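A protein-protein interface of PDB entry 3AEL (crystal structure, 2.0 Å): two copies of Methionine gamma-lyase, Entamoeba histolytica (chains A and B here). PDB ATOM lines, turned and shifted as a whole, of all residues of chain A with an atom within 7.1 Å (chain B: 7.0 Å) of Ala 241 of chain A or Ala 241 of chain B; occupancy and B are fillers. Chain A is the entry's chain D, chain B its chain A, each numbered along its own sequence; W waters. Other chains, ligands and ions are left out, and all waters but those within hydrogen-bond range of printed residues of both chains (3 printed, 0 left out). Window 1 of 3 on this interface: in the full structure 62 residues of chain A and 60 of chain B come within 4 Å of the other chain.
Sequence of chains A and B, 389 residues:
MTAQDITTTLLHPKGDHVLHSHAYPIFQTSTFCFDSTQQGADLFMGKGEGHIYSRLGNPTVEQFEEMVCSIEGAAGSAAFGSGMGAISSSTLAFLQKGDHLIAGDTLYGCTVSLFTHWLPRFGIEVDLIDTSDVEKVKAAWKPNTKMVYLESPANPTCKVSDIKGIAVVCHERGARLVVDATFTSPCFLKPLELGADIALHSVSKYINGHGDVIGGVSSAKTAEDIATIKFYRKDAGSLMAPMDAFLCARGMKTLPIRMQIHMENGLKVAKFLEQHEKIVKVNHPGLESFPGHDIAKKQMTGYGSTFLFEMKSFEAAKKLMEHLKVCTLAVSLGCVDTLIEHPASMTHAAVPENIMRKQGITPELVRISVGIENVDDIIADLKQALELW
The side-chain carboxylate (OD2) of Asp 244 of chain B sits close to the side-chain amide oxygen (OE1) of Gln 28 of chain A, 3.0 Å away. OD2 of Asp 244 of chain A sits close to OE1 of Gln 28 of chain B (2.9 Å).
Gln 28 of chain A touches Leu 247 of chain B, and with the chains exchanged Leu 247 of chain A touches Gln 28 of chain B. Gly 81 of chain A touches Leu 239 of chain B, and with the chains exchanged Leu 239 of chain A touches Gly 81 of chain B. Ala 241 of chain A touches its own counterpart, Ala 241 of chain B. Ala 241 of chain A touches Asp 244 of chain B, and with the chains exchanged Asp 244 of chain A touches Ala 241 of chain B.
Water W1 lies within hydrogen-bond range of NE2 of Gln 28 of chain A (2.6 Å), OD2 of Asp 244 of chain B (2.9 Å) and N of Met 243 of chain A (2.9 Å). Water W3 lies within hydrogen-bond range of the side-chain amide nitrogen (NE2) of Gln 28 of chain B, the side-chain carboxylate (OD2) of Asp 244 of chain A and the backbone NH (N) of Met 243 of chain B. Water W2 lies within hydrogen-bond range of O of Leu 239 of chain A and O of Leu 239 of chain B.
Of the 18 printed residues of chain B, 7 touch a printed residue of chain A. Hydrophobic or aromatic side chains of chain B within 4 Å of the printed part of chain A: Ile 214, Leu 239, Ala 241 and Leu 247. Of the 19 printed residues of chain A, 8 touch a printed residue of chain B. Among the printed residues, 12 pairs touch across the chains. Among the printed residues, no Asp or Glu carboxylate lies within 4 Å of a Lys or Arg side-chain nitrogen of the other chain.
Gln 28 of chain A touches Leu 247 of chain B (OE1 to CD1, 3.7 Å). O of Gly 81 of chain A touches CD1 of Leu 239 of chain B, 3.8 Å away. CG2 of Val 213 of chain A touches OE1 of Gln 28 of chain B (3.9 Å). CG2 of Ile 214 of chain A touches CD1 of Leu 239 of chain B, at 3.8 Å. Gly 81 of chain B touches Leu 239 of chain A (O to CD1, 3.9 Å). Ile 214 of chain B touches Leu 239 of chain A (CG2 to CD1, 3.8 Å). Ala 241 of chain A touches Ala 241 of chain B (CB to CB, 3.6 Å). Ala 241 of chain A touches Asp 244 of chain B (CB to OD1, 3.3 Å). Asp 244 of chain A touches Ala 241 of chain B (OD1 to CB, 3.4 Å). Gln 28 of chain B touches Leu 247 of chain A.
Of chain B, only Ala 241 (3.6 Å) and Asp 244 (3.3 Å) come within 4 Å of Ala 241 of chain A. Of chain A, only Ala 241 and Asp 244 come within 4 Å of Ala 241 of chain B. Of the printed residues of chain A, Gln 28 of chain B touches Val 213, Asp 244 and Leu 247. Of the printed residues of chain B, Ile 214 of chain A touches Leu 239 (3.8 Å). Of the printed residues of chain A, Leu 239 of chain B touches Gly 81 and Ile 214. Of the printed residues of chain B, Val 213 of chain A touches Gln 28 (3.9 Å). Printed residues of chain A within 4 Å of Ile 214 of chain B: Leu 239. Ile 26 of chain A touches none of the printed residues of chain B. Phe 27 of chain A touches none of the printed residues of chain B. The nearest residue of chain B that does not touch Ala 241 of chain A is Met 243 of chain B (6.3 Å).
N of Gly 81 of chain A sits close to O of Leu 239 of chain A, at 3.3 Å. N of Gly 81 of chain B lies close to O of Leu 239 of chain B, at 3.2 Å.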
ATOM      1  N   ILE A  26     -22.412  33.154   9.798  1.00  0.00           N
ATOM      2  CA  ILE A  26     -21.248  32.947   8.941  1.00  0.00           C
ATOM      3  C   ILE A  26     -21.268  34.063   7.921  1.00  0.00           C
ATOM      4  O   ILE A  26     -22.120  34.080   7.018  1.00  0.00           O
ATOM      5  CB  ILE A  26     -21.284  31.584   8.196  1.00  0.00           C
ATOM      6  CG1 ILE A  26     -21.547  30.429   9.188  1.00  0.00           C
ATOM      7  CG2 ILE A  26     -19.989  31.381   7.350  1.00  0.00           C
ATOM      8  CD1 ILE A  26     -21.824  29.082   8.523  1.00  0.00           C
ATOM      9  N   PHE A  27     -20.321  34.994   8.046  1.00  0.00           N
ATOM     10  CA  PHE A  27     -20.266  36.092   7.078  1.00  0.00           C
ATOM     11  C   PHE A  27     -19.523  35.680   5.835  1.00  0.00           C
ATOM     12  O   PHE A  27     -18.347  36.057   5.623  1.00  0.00           O
ATOM     13  CB  PHE A  27     -19.674  37.368   7.701  1.00  0.00           C
ATOM     14  CG  PHE A  27     -20.643  38.088   8.572  1.00  0.00           C
ATOM     15  CD1 PHE A  27     -21.306  39.219   8.109  1.00  0.00           C
ATOM     16  CD2 PHE A  27     -20.918  37.605   9.854  1.00  0.00           C
ATOM     17  CE1 PHE A  27     -22.250  39.892   8.938  1.00  0.00           C
ATOM     18  CE2 PHE A  27     -21.861  38.251  10.699  1.00  0.00           C
ATOM     19  CZ  PHE A  27     -22.519  39.398  10.235  1.00  0.00           C
ATOM     20  N   GLN A  28     -20.201  34.879   5.009  1.00  0.00           N
ATOM     21  CA  GLN A  28     -19.644  34.434   3.750  1.00  0.00           C
ATOM     22  C   GLN A  28     -19.726  35.559   2.701  1.00  0.00           C
ATOM     23  O   GLN A  28     -20.557  35.543   1.750  1.00  0.00           O
ATOM     24  CB  GLN A  28     -20.361  33.137   3.308  1.00  0.00           C
ATOM     25  CG  GLN A  28     -19.739  32.424   2.109  1.00  0.00           C
ATOM     26  CD  GLN A  28     -18.387  31.777   2.382  1.00  0.00           C
ATOM     27  OE1 GLN A  28     -17.396  32.016   1.653  1.00  0.00           O
ATOM     28  NE2 GLN A  28     -18.326  30.978   3.409  1.00  0.00           N
ATOM     29  N   ASN A  58     -13.136  40.182   8.943  1.00  0.00           N
ATOM     30  CA  ASN A  58     -14.392  39.471   8.785  1.00  0.00           C
ATOM     31  C   ASN A  58     -15.000  39.163  10.158  1.00  0.00           C
ATOM     32  O   ASN A  58     -14.332  38.633  11.018  1.00  0.00           O
ATOM     33  CB  ASN A  58     -14.156  38.185   8.009  1.00  0.00           C
ATOM     34  CG  ASN A  58     -15.438  37.386   7.814  1.00  0.00           C
ATOM     35  OD1 ASN A  58     -15.885  36.666   8.721  1.00  0.00           O
ATOM     36  ND2 ASN A  58     -16.037  37.517   6.634  1.00  0.00           N
ATOM     37  N   THR A  60     -17.032  36.891  11.431  1.00  0.00           N
ATOM     38  CA  THR A  60     -17.019  35.506  11.898  1.00  0.00           C
ATOM     39  C   THR A  60     -15.589  35.116  12.317  1.00  0.00           C
ATOM     40  O   THR A  60     -15.369  34.481  13.373  1.00  0.00           O
ATOM     41  CB  THR A  60     -17.538  34.541  10.789  1.00  0.00           C
ATOM     42  OG1 THR A  60     -18.796  35.004  10.321  1.00  0.00           O
ATOM     43  CG2 THR A  60     -17.681  33.102  11.318  1.00  0.00           C
ATOM     44  N   VAL A  61     -14.610  35.537  11.524  1.00  0.00           N
ATOM     45  CA  VAL A  61     -13.214  35.255  11.838  1.00  0.00           C
ATOM     46  C   VAL A  61     -12.797  36.021  13.123  1.00  0.00           C
ATOM     47  O   VAL A  61     -12.100  35.466  13.994  1.00  0.00           O
ATOM     48  CB  VAL A  61     -12.285  35.639  10.659  1.00  0.00           C
ATOM     49  CG1 VAL A  61     -10.800  35.398  11.059  1.00  0.00           C
ATOM     50  CG2 VAL A  61     -12.682  34.874   9.382  1.00  0.00           C
ATOM     51  N   PHE A  80      -5.477  32.602  10.525  1.00  0.00           N
ATOM     52  CA  PHE A  80      -4.811  32.349   9.240  1.00  0.00           C
ATOM     53  C   PHE A  80      -5.369  31.086   8.590  1.00  0.00           C
ATOM     54  O   PHE A  80      -6.050  30.287   9.238  1.00  0.00           O
ATOM     55  CB  PHE A  80      -3.310  32.111   9.506  1.00  0.00           C
ATOM     56  CG  PHE A  80      -2.609  33.307  10.079  1.00  0.00           C
ATOM     57  CD1 PHE A  80      -2.088  34.295   9.230  1.00  0.00           C
ATOM     58  CD2 PHE A  80      -2.511  33.481  11.459  1.00  0.00           C
ATOM     59  CE1 PHE A  80      -1.419  35.398   9.769  1.00  0.00           C
ATOM     60  CE2 PHE A  80      -1.862  34.592  11.987  1.00  0.00           C
ATOM     61  CZ  PHE A  80      -1.348  35.559  11.134  1.00  0.00           C
ATOM     62  N   GLY A  81      -5.017  30.870   7.337  1.00  0.00           N
ATOM     63  CA  GLY A  81      -5.472  29.706   6.604  1.00  0.00           C
ATOM     64  C   GLY A  81      -4.786  28.401   6.994  1.00  0.00           C
ATOM     65  O   GLY A  81      -5.244  27.352   6.605  1.00  0.00           O
ATOM     66  N   VAL A 213     -10.757  20.959   9.384  1.00  0.00           N
ATOM     67  CA  VAL A 213     -10.322  22.326   9.072  1.00  0.00           C
ATOM     68  C   VAL A 213      -8.788  22.396   9.141  1.00  0.00           C
ATOM     69  O   VAL A 213      -8.157  21.779  10.007  1.00  0.00           O
ATOM     70  CB  VAL A 213     -10.894  23.390  10.079  1.00  0.00           C
ATOM     71  CG1 VAL A 213     -10.314  24.798   9.774  1.00  0.00           C
ATOM     72  CG2 VAL A 213     -12.431  23.448  10.033  1.00  0.00           C
ATOM     73  N   ILE A 214      -8.200  23.148   8.215  1.00  0.00           N
ATOM     74  CA  ILE A 214      -6.852  23.611   8.373  1.00  0.00           C
ATOM     75  C   ILE A 214      -6.857  25.116   8.681  1.00  0.00           C
ATOM     76  O   ILE A 214      -7.513  25.891   7.995  1.00  0.00           O
ATOM     77  CB  ILE A 214      -5.982  23.261   7.143  1.00  0.00           C
ATOM     78  CG1 ILE A 214      -5.767  21.726   7.132  1.00  0.00           C
ATOM     79  CG2 ILE A 214      -4.617  24.033   7.249  1.00  0.00           C
ATOM     80  CD1 ILE A 214      -4.904  21.197   6.005  1.00  0.00           C
ATOM     81  N   LEU A 239      -5.469  33.744   4.980  1.00  0.00           N
ATOM     82  CA  LEU A 239      -6.685  34.077   5.740  1.00  0.00           C
ATOM     83  C   LEU A 239      -7.432  32.810   6.139  1.00  0.00           C
ATOM     84  O   LEU A 239      -7.436  31.817   5.379  1.00  0.00           O
ATOM     85  CB  LEU A 239      -7.641  34.891   4.860  1.00  0.00           C
ATOM     86  CG  LEU A 239      -7.018  36.068   4.115  1.00  0.00           C
ATOM     87  CD1 LEU A 239      -8.062  36.745   3.191  1.00  0.00           C
ATOM     88  CD2 LEU A 239      -6.427  37.075   5.163  1.00  0.00           C
ATOM     89  N   MET A 240      -8.116  32.884   7.281  1.00  0.00           N
ATOM     90  CA  MET A 240      -9.104  31.871   7.641  1.00  0.00           C
ATOM     91  C   MET A 240     -10.432  32.201   6.942  1.00  0.00           C
ATOM     92  O   MET A 240     -10.956  33.316   7.061  1.00  0.00           O
ATOM     93  CB  MET A 240      -9.276  31.792   9.171  1.00  0.00           C
ATOM     94  CG  MET A 240     -10.353  30.764   9.627  1.00  0.00           C
ATOM     95  SD  MET A 240     -10.289  30.697  11.403  1.00  0.00           S
ATOM     96  CE  MET A 240      -8.947  29.547  11.738  1.00  0.00           C
ATOM     97  N   ALA A 241     -10.962  31.231   6.209  1.00  0.00           N
ATOM     98  CA  ALA A 241     -12.261  31.373   5.556  1.00  0.00           C
ATOM     99  C   ALA A 241     -13.390  31.478   6.583  1.00  0.00           C
ATOM    100  O   ALA A 241     -13.318  30.832   7.627  1.00  0.00           O
ATOM    101  CB  ALA A 241     -12.501  30.174   4.606  1.00  0.00           C
ATOM    102  N   PRO A 242     -14.428  32.294   6.298  1.00  0.00           N
ATOM    103  CA  PRO A 242     -15.521  32.447   7.266  1.00  0.00           C
ATOM    104  C   PRO A 242     -16.120  31.101   7.669  1.00  0.00           C
ATOM    105  O   PRO A 242     -16.440  30.928   8.834  1.00  0.00           O
ATOM    106  CB  PRO A 242     -16.583  33.275   6.521  1.00  0.00           C
ATOM    107  CG  PRO A 242     -15.885  33.867   5.334  1.00  0.00           C
ATOM    108  CD  PRO A 242     -14.649  33.062   5.045  1.00  0.00           C
ATOM    109  N   MET A 243     -16.283  30.166   6.726  1.00  0.00           N
ATOM    110  CA  MET A 243     -16.854  28.853   7.086  1.00  0.00           C
ATOM    111  C   MET A 243     -15.921  28.108   8.057  1.00  0.00           C
ATOM    112  O   MET A 243     -16.363  27.533   9.067  1.00  0.00           O
ATOM    113  CB  MET A 243     -17.142  27.997   5.814  1.00  0.00           C
ATOM    114  CG  MET A 243     -17.578  26.552   6.109  1.00  0.00           C
ATOM    115  SD  MET A 243     -19.115  26.546   7.007  1.00  0.00           S
ATOM    116  CE  MET A 243     -20.224  27.133   5.771  1.00  0.00           C
ATOM    117  N   ASP A 244     -14.620  28.150   7.774  1.00  0.00           N
ATOM    118  CA  ASP A 244     -13.636  27.518   8.667  1.00  0.00           C
ATOM    119  C   ASP A 244     -13.597  28.148  10.057  1.00  0.00           C
ATOM    120  O   ASP A 244     -13.435  27.440  11.063  1.00  0.00           O
ATOM    121  CB  ASP A 244     -12.254  27.517   8.028  1.00  0.00           C
ATOM    122  CG  ASP A 244     -12.126  26.468   6.925  1.00  0.00           C
ATOM    123  OD1 ASP A 244     -11.079  26.467   6.249  1.00  0.00           O
ATOM    124  OD2 ASP A 244     -13.066  25.642   6.735  1.00  0.00           O
ATOM    125  N   ALA A 245     -13.763  29.467  10.123  1.00  0.00           N
ATOM    126  CA  ALA A 245     -13.825  30.153  11.434  1.00  0.00           C
ATOM    127  C   ALA A 245     -15.084  29.769  12.200  1.00  0.00           C
ATOM    128  O   ALA A 245     -15.057  29.678  13.422  1.00  0.00           O
ATOM    129  CB  ALA A 245     -13.779  31.677  11.277  1.00  0.00           C
ATOM    130  N   PHE A 246     -16.204  29.642  11.493  1.00  0.00           N
ATOM    131  CA  PHE A 246     -17.428  29.121  12.105  1.00  0.00           C
ATOM    132  C   PHE A 246     -17.123  27.725  12.666  1.00  0.00           C
ATOM    133  O   PHE A 246     -17.443  27.429  13.835  1.00  0.00           O
ATOM    134  CB  PHE A 246     -18.571  29.086  11.072  1.00  0.00           C
ATOM    135  CG  PHE A 246     -19.732  28.213  11.485  1.00  0.00           C
ATOM    136  CD1 PHE A 246     -20.792  28.749  12.240  1.00  0.00           C
ATOM    137  CD2 PHE A 246     -19.784  26.890  11.082  1.00  0.00           C
ATOM    138  CE1 PHE A 246     -21.898  27.944  12.640  1.00  0.00           C
ATOM    139  CE2 PHE A 246     -20.865  26.081  11.464  1.00  0.00           C
ATOM    140  CZ  PHE A 246     -21.934  26.632  12.255  1.00  0.00           C
ATOM    141  N   LEU A 247     -16.459  26.879  11.877  1.00  0.00           N
ATOM    142  CA  LEU A 247     -16.151  25.515  12.355  1.00  0.00           C
ATOM    143  C   LEU A 247     -15.134  25.494  13.502  1.00  0.00           C
ATOM    144  O   LEU A 247     -15.250  24.687  14.424  1.00  0.00           O
ATOM    145  CB  LEU A 247     -15.690  24.610  11.214  1.00  0.00           C
ATOM    146  CG  LEU A 247     -16.765  24.221  10.162  1.00  0.00           C
ATOM    147  CD1 LEU A 247     -16.095  23.524   8.968  1.00  0.00           C
ATOM    148  CD2 LEU A 247     -17.859  23.302  10.796  1.00  0.00           C
ATOM    149  N   ILE B  26     -17.422  18.373  -1.299  1.00  0.00           N
ATOM    150  CA  ILE B  26     -16.603  19.307  -0.542  1.00  0.00           C
ATOM    151  C   ILE B  26     -15.811  18.465   0.430  1.00  0.00           C
ATOM    152  O   ILE B  26     -16.396  17.862   1.388  1.00  0.00           O
ATOM    153  CB  ILE B  26     -17.449  20.348   0.207  1.00  0.00           C
ATOM    154  CG1 ILE B  26     -18.465  21.043  -0.724  1.00  0.00           C
ATOM    155  CG2 ILE B  26     -16.536  21.406   0.908  1.00  0.00           C
ATOM    156  CD1 ILE B  26     -19.511  21.864   0.056  1.00  0.00           C
ATOM    157  N   PHE B  27     -14.492  18.406   0.191  1.00  0.00           N
ATOM    158  CA  PHE B  27     -13.610  17.634   1.084  1.00  0.00           C
ATOM    159  C   PHE B  27     -13.195  18.476   2.282  1.00  0.00           C
ATOM    160  O   PHE B  27     -12.061  18.986   2.348  1.00  0.00           O
ATOM    161  CB  PHE B  27     -12.401  17.072   0.310  1.00  0.00           C
ATOM    162  CG  PHE B  27     -12.742  15.850  -0.488  1.00  0.00           C
ATOM    163  CD1 PHE B  27     -12.480  14.572   0.025  1.00  0.00           C
ATOM    164  CD2 PHE B  27     -13.370  15.972  -1.724  1.00  0.00           C
ATOM    165  CE1 PHE B  27     -12.815  13.433  -0.707  1.00  0.00           C
ATOM    166  CE2 PHE B  27     -13.720  14.844  -2.452  1.00  0.00           C
ATOM    167  CZ  PHE B  27     -13.444  13.579  -1.953  1.00  0.00           C
ATOM    168  N   GLN B  28     -14.159  18.693   3.177  1.00  0.00           N
ATOM    169  CA  GLN B  28     -13.933  19.422   4.413  1.00  0.00           C
ATOM    170  C   GLN B  28     -13.186  18.510   5.396  1.00  0.00           C
ATOM    171  O   GLN B  28     -13.780  17.971   6.360  1.00  0.00           O
ATOM    172  CB  GLN B  28     -15.271  19.899   5.016  1.00  0.00           C
ATOM    173  CG  GLN B  28     -15.139  20.883   6.193  1.00  0.00           C
ATOM    174  CD  GLN B  28     -14.580  22.271   5.781  1.00  0.00           C
ATOM    175  OE1 GLN B  28     -13.628  22.775   6.395  1.00  0.00           O
ATOM    176  NE2 GLN B  28     -15.179  22.887   4.770  1.00  0.00           N
ATOM    177  N   ASN B  58      -5.816  19.265  -1.645  1.00  0.00           N
ATOM    178  CA  ASN B  58      -7.188  18.916  -1.279  1.00  0.00           C
ATOM    179  C   ASN B  58      -7.981  18.657  -2.563  1.00  0.00           C
ATOM    180  O   ASN B  58      -7.894  19.451  -3.487  1.00  0.00           O
ATOM    181  CB  ASN B  58      -7.799  20.057  -0.463  1.00  0.00           C
ATOM    182  CG  ASN B  58      -9.289  19.827  -0.157  1.00  0.00           C
ATOM    183  OD1 ASN B  58     -10.160  20.060  -1.002  1.00  0.00           O
ATOM    184  ND2 ASN B  58      -9.579  19.352   1.056  1.00  0.00           N
ATOM    185  N   THR B  60     -11.056  19.041  -3.540  1.00  0.00           N
ATOM    186  CA  THR B  60     -11.992  20.058  -4.009  1.00  0.00           C
ATOM    187  C   THR B  60     -11.217  21.245  -4.553  1.00  0.00           C
ATOM    188  O   THR B  60     -11.564  21.846  -5.582  1.00  0.00           O
ATOM    189  CB  THR B  60     -12.922  20.500  -2.857  1.00  0.00           C
ATOM    190  OG1 THR B  60     -13.560  19.340  -2.348  1.00  0.00           O
ATOM    191  CG2 THR B  60     -13.978  21.514  -3.325  1.00  0.00           C
ATOM    192  N   VAL B  61     -10.154  21.610  -3.849  1.00  0.00           N
ATOM    193  CA  VAL B  61      -9.312  22.722  -4.302  1.00  0.00           C
ATOM    194  C   VAL B  61      -8.626  22.387  -5.643  1.00  0.00           C
ATOM    195  O   VAL B  61      -8.573  23.217  -6.559  1.00  0.00           O
ATOM    196  CB  VAL B  61      -8.262  23.071  -3.217  1.00  0.00           C
ATOM    197  CG1 VAL B  61      -7.309  24.199  -3.707  1.00  0.00           C
ATOM    198  CG2 VAL B  61      -8.979  23.491  -1.982  1.00  0.00           C
ATOM    199  N   PHE B  80      -5.197  29.906  -3.694  1.00  0.00           N
ATOM    200  CA  PHE B  80      -4.738  30.540  -2.418  1.00  0.00           C
ATOM    201  C   PHE B  80      -5.918  31.137  -1.653  1.00  0.00           C
ATOM    202  O   PHE B  80      -7.000  31.287  -2.217  1.00  0.00           O
ATOM    203  CB  PHE B  80      -3.764  31.687  -2.777  1.00  0.00           C
ATOM    204  CG  PHE B  80      -2.525  31.213  -3.489  1.00  0.00           C
ATOM    205  CD1 PHE B  80      -1.415  30.795  -2.762  1.00  0.00           C
ATOM    206  CD2 PHE B  80      -2.489  31.116  -4.859  1.00  0.00           C
ATOM    207  CE1 PHE B  80      -0.269  30.314  -3.413  1.00  0.00           C
ATOM    208  CE2 PHE B  80      -1.323  30.653  -5.532  1.00  0.00           C
ATOM    209  CZ  PHE B  80      -0.232  30.244  -4.798  1.00  0.00           C
ATOM    210  N   GLY B  81      -5.678  31.507  -0.384  1.00  0.00           N
ATOM    211  CA  GLY B  81      -6.644  32.167   0.467  1.00  0.00           C
ATOM    212  C   GLY B  81      -7.062  33.554  -0.020  1.00  0.00           C
ATOM    213  O   GLY B  81      -8.080  34.060   0.421  1.00  0.00           O
ATOM    214  N   ILE B 214     -13.160  35.287  -0.714  1.00  0.00           N
ATOM    215  CA  ILE B 214     -11.841  35.850  -1.038  1.00  0.00           C
ATOM    216  C   ILE B 214     -10.915  34.697  -1.424  1.00  0.00           C
ATOM    217  O   ILE B 214     -10.837  33.685  -0.710  1.00  0.00           O
ATOM    218  CB  ILE B 214     -11.326  36.733   0.124  1.00  0.00           C
ATOM    219  CG1 ILE B 214     -12.240  38.013   0.183  1.00  0.00           C
ATOM    220  CG2 ILE B 214      -9.821  37.104  -0.120  1.00  0.00           C
ATOM    221  CD1 ILE B 214     -11.770  39.078   1.114  1.00  0.00           C
ATOM    222  N   LEU B 239      -3.929  29.238   1.937  1.00  0.00           N
ATOM    223  CA  LEU B 239      -4.675  28.170   1.272  1.00  0.00           C
ATOM    224  C   LEU B 239      -6.099  28.601   0.949  1.00  0.00           C
ATOM    225  O   LEU B 239      -6.738  29.341   1.724  1.00  0.00           O
ATOM    226  CB  LEU B 239      -4.771  26.960   2.230  1.00  0.00           C
ATOM    227  CG  LEU B 239      -3.436  26.427   2.770  1.00  0.00           C
ATOM    228  CD1 LEU B 239      -3.713  25.326   3.769  1.00  0.00           C
ATOM    229  CD2 LEU B 239      -2.514  25.920   1.626  1.00  0.00           C
ATOM    230  N   MET B 240      -6.646  28.044  -0.109  1.00  0.00           N
ATOM    231  CA  MET B 240      -8.078  28.167  -0.362  1.00  0.00           C
ATOM    232  C   MET B 240      -8.775  27.046   0.419  1.00  0.00           C
ATOM    233  O   MET B 240      -8.435  25.862   0.226  1.00  0.00           O
ATOM    234  CB  MET B 240      -8.373  28.012  -1.853  1.00  0.00           C
ATOM    235  CG  MET B 240      -9.896  28.029  -2.174  1.00  0.00           C
ATOM    236  SD  MET B 240     -10.136  28.124  -3.968  1.00  0.00           S
ATOM    237  CE  MET B 240      -9.612  29.814  -4.369  1.00  0.00           C
ATOM    238  N   ALA B 241      -9.763  27.417   1.252  1.00  0.00           N
ATOM    239  CA  ALA B 241     -10.562  26.456   2.017  1.00  0.00           C
ATOM    240  C   ALA B 241     -11.416  25.602   1.075  1.00  0.00           C
ATOM    241  O   ALA B 241     -11.839  26.076   0.015  1.00  0.00           O
ATOM    242  CB  ALA B 241     -11.466  27.175   2.991  1.00  0.00           C
ATOM    243  N   PRO B 242     -11.692  24.342   1.475  1.00  0.00           N
ATOM    244  CA  PRO B 242     -12.520  23.460   0.640  1.00  0.00           C
ATOM    245  C   PRO B 242     -13.895  24.075   0.315  1.00  0.00           C
ATOM    246  O   PRO B 242     -14.346  23.954  -0.822  1.00  0.00           O
ATOM    247  CB  PRO B 242     -12.713  22.194   1.518  1.00  0.00           C
ATOM    248  CG  PRO B 242     -11.511  22.213   2.462  1.00  0.00           C
ATOM    249  CD  PRO B 242     -11.072  23.641   2.633  1.00  0.00           C
ATOM    250  N   MET B 243     -14.566  24.693   1.290  1.00  0.00           N
ATOM    251  CA  MET B 243     -15.862  25.326   0.995  1.00  0.00           C
ATOM    252  C   MET B 243     -15.681  26.453  -0.043  1.00  0.00           C
ATOM    253  O   MET B 243     -16.488  26.582  -0.960  1.00  0.00           O
ATOM    254  CB  MET B 243     -16.518  25.875   2.255  1.00  0.00           C
ATOM    255  CG  MET B 243     -17.809  26.663   2.012  1.00  0.00           C
ATOM    256  SD  MET B 243     -19.082  25.590   1.333  1.00  0.00           S
ATOM    257  CE  MET B 243     -19.366  24.561   2.739  1.00  0.00           C
ATOM    258  N   ASP B 244     -14.646  27.273   0.142  1.00  0.00           N
ATOM    259  CA  ASP B 244     -14.421  28.383  -0.783  1.00  0.00           C
ATOM    260  C   ASP B 244     -14.102  27.881  -2.170  1.00  0.00           C
ATOM    261  O   ASP B 244     -14.518  28.488  -3.173  1.00  0.00           O
ATOM    262  CB  ASP B 244     -13.314  29.318  -0.262  1.00  0.00           C
ATOM    263  CG  ASP B 244     -13.812  30.240   0.883  1.00  0.00           C
ATOM    264  OD1 ASP B 244     -12.982  30.965   1.474  1.00  0.00           O
ATOM    265  OD2 ASP B 244     -15.039  30.268   1.179  1.00  0.00           O
ATOM    266  N   ALA B 245     -13.353  26.781  -2.249  1.00  0.00           N
ATOM    267  CA  ALA B 245     -13.049  26.213  -3.576  1.00  0.00           C
ATOM    268  C   ALA B 245     -14.316  25.667  -4.268  1.00  0.00           C
ATOM    269  O   ALA B 245     -14.483  25.813  -5.497  1.00  0.00           O
ATOM    270  CB  ALA B 245     -11.928  25.090  -3.512  1.00  0.00           C
ATOM    271  N   PHE B 246     -15.176  25.035  -3.488  1.00  0.00           N
ATOM    272  CA  PHE B 246     -16.482  24.592  -3.998  1.00  0.00           C
ATOM    273  C   PHE B 246     -17.244  25.822  -4.540  1.00  0.00           C
ATOM    274  O   PHE B 246     -17.788  25.776  -5.623  1.00  0.00           O
ATOM    275  CB  PHE B 246     -17.273  23.952  -2.878  1.00  0.00           C
ATOM    276  CG  PHE B 246     -18.753  23.827  -3.146  1.00  0.00           C
ATOM    277  CD1 PHE B 246     -19.258  22.737  -3.875  1.00  0.00           C
ATOM    278  CD2 PHE B 246     -19.654  24.766  -2.616  1.00  0.00           C
ATOM    279  CE1 PHE B 246     -20.647  22.619  -4.112  1.00  0.00           C
ATOM    280  CE2 PHE B 246     -21.029  24.663  -2.845  1.00  0.00           C
ATOM    281  CZ  PHE B 246     -21.527  23.591  -3.579  1.00  0.00           C
ATOM    282  N   LEU B 247     -17.288  26.909  -3.775  1.00  0.00           N
ATOM    283  CA  LEU B 247     -17.969  28.145  -4.267  1.00  0.00           C
ATOM    284  C   LEU B 247     -17.283  28.777  -5.461  1.00  0.00           C
ATOM    285  O   LEU B 247     -17.976  29.276  -6.364  1.00  0.00           O
ATOM    286  CB  LEU B 247     -18.076  29.191  -3.148  1.00  0.00           C
ATOM    287  CG  LEU B 247     -18.985  28.736  -1.997  1.00  0.00           C
ATOM    288  CD1 LEU B 247     -18.862  29.688  -0.765  1.00  0.00           C
ATOM    289  CD2 LEU B 247     -20.452  28.679  -2.486  1.00  0.00           C
HETATM  290  O   HOH W   1     -15.935  30.025   3.877  1.00  0.00           O
HETATM  291  O   HOH W   2      -5.545  31.173   3.473  1.00  0.00           O
HETATM  292  O   HOH W   3     -14.081  25.191   4.168  1.00  0.00           O
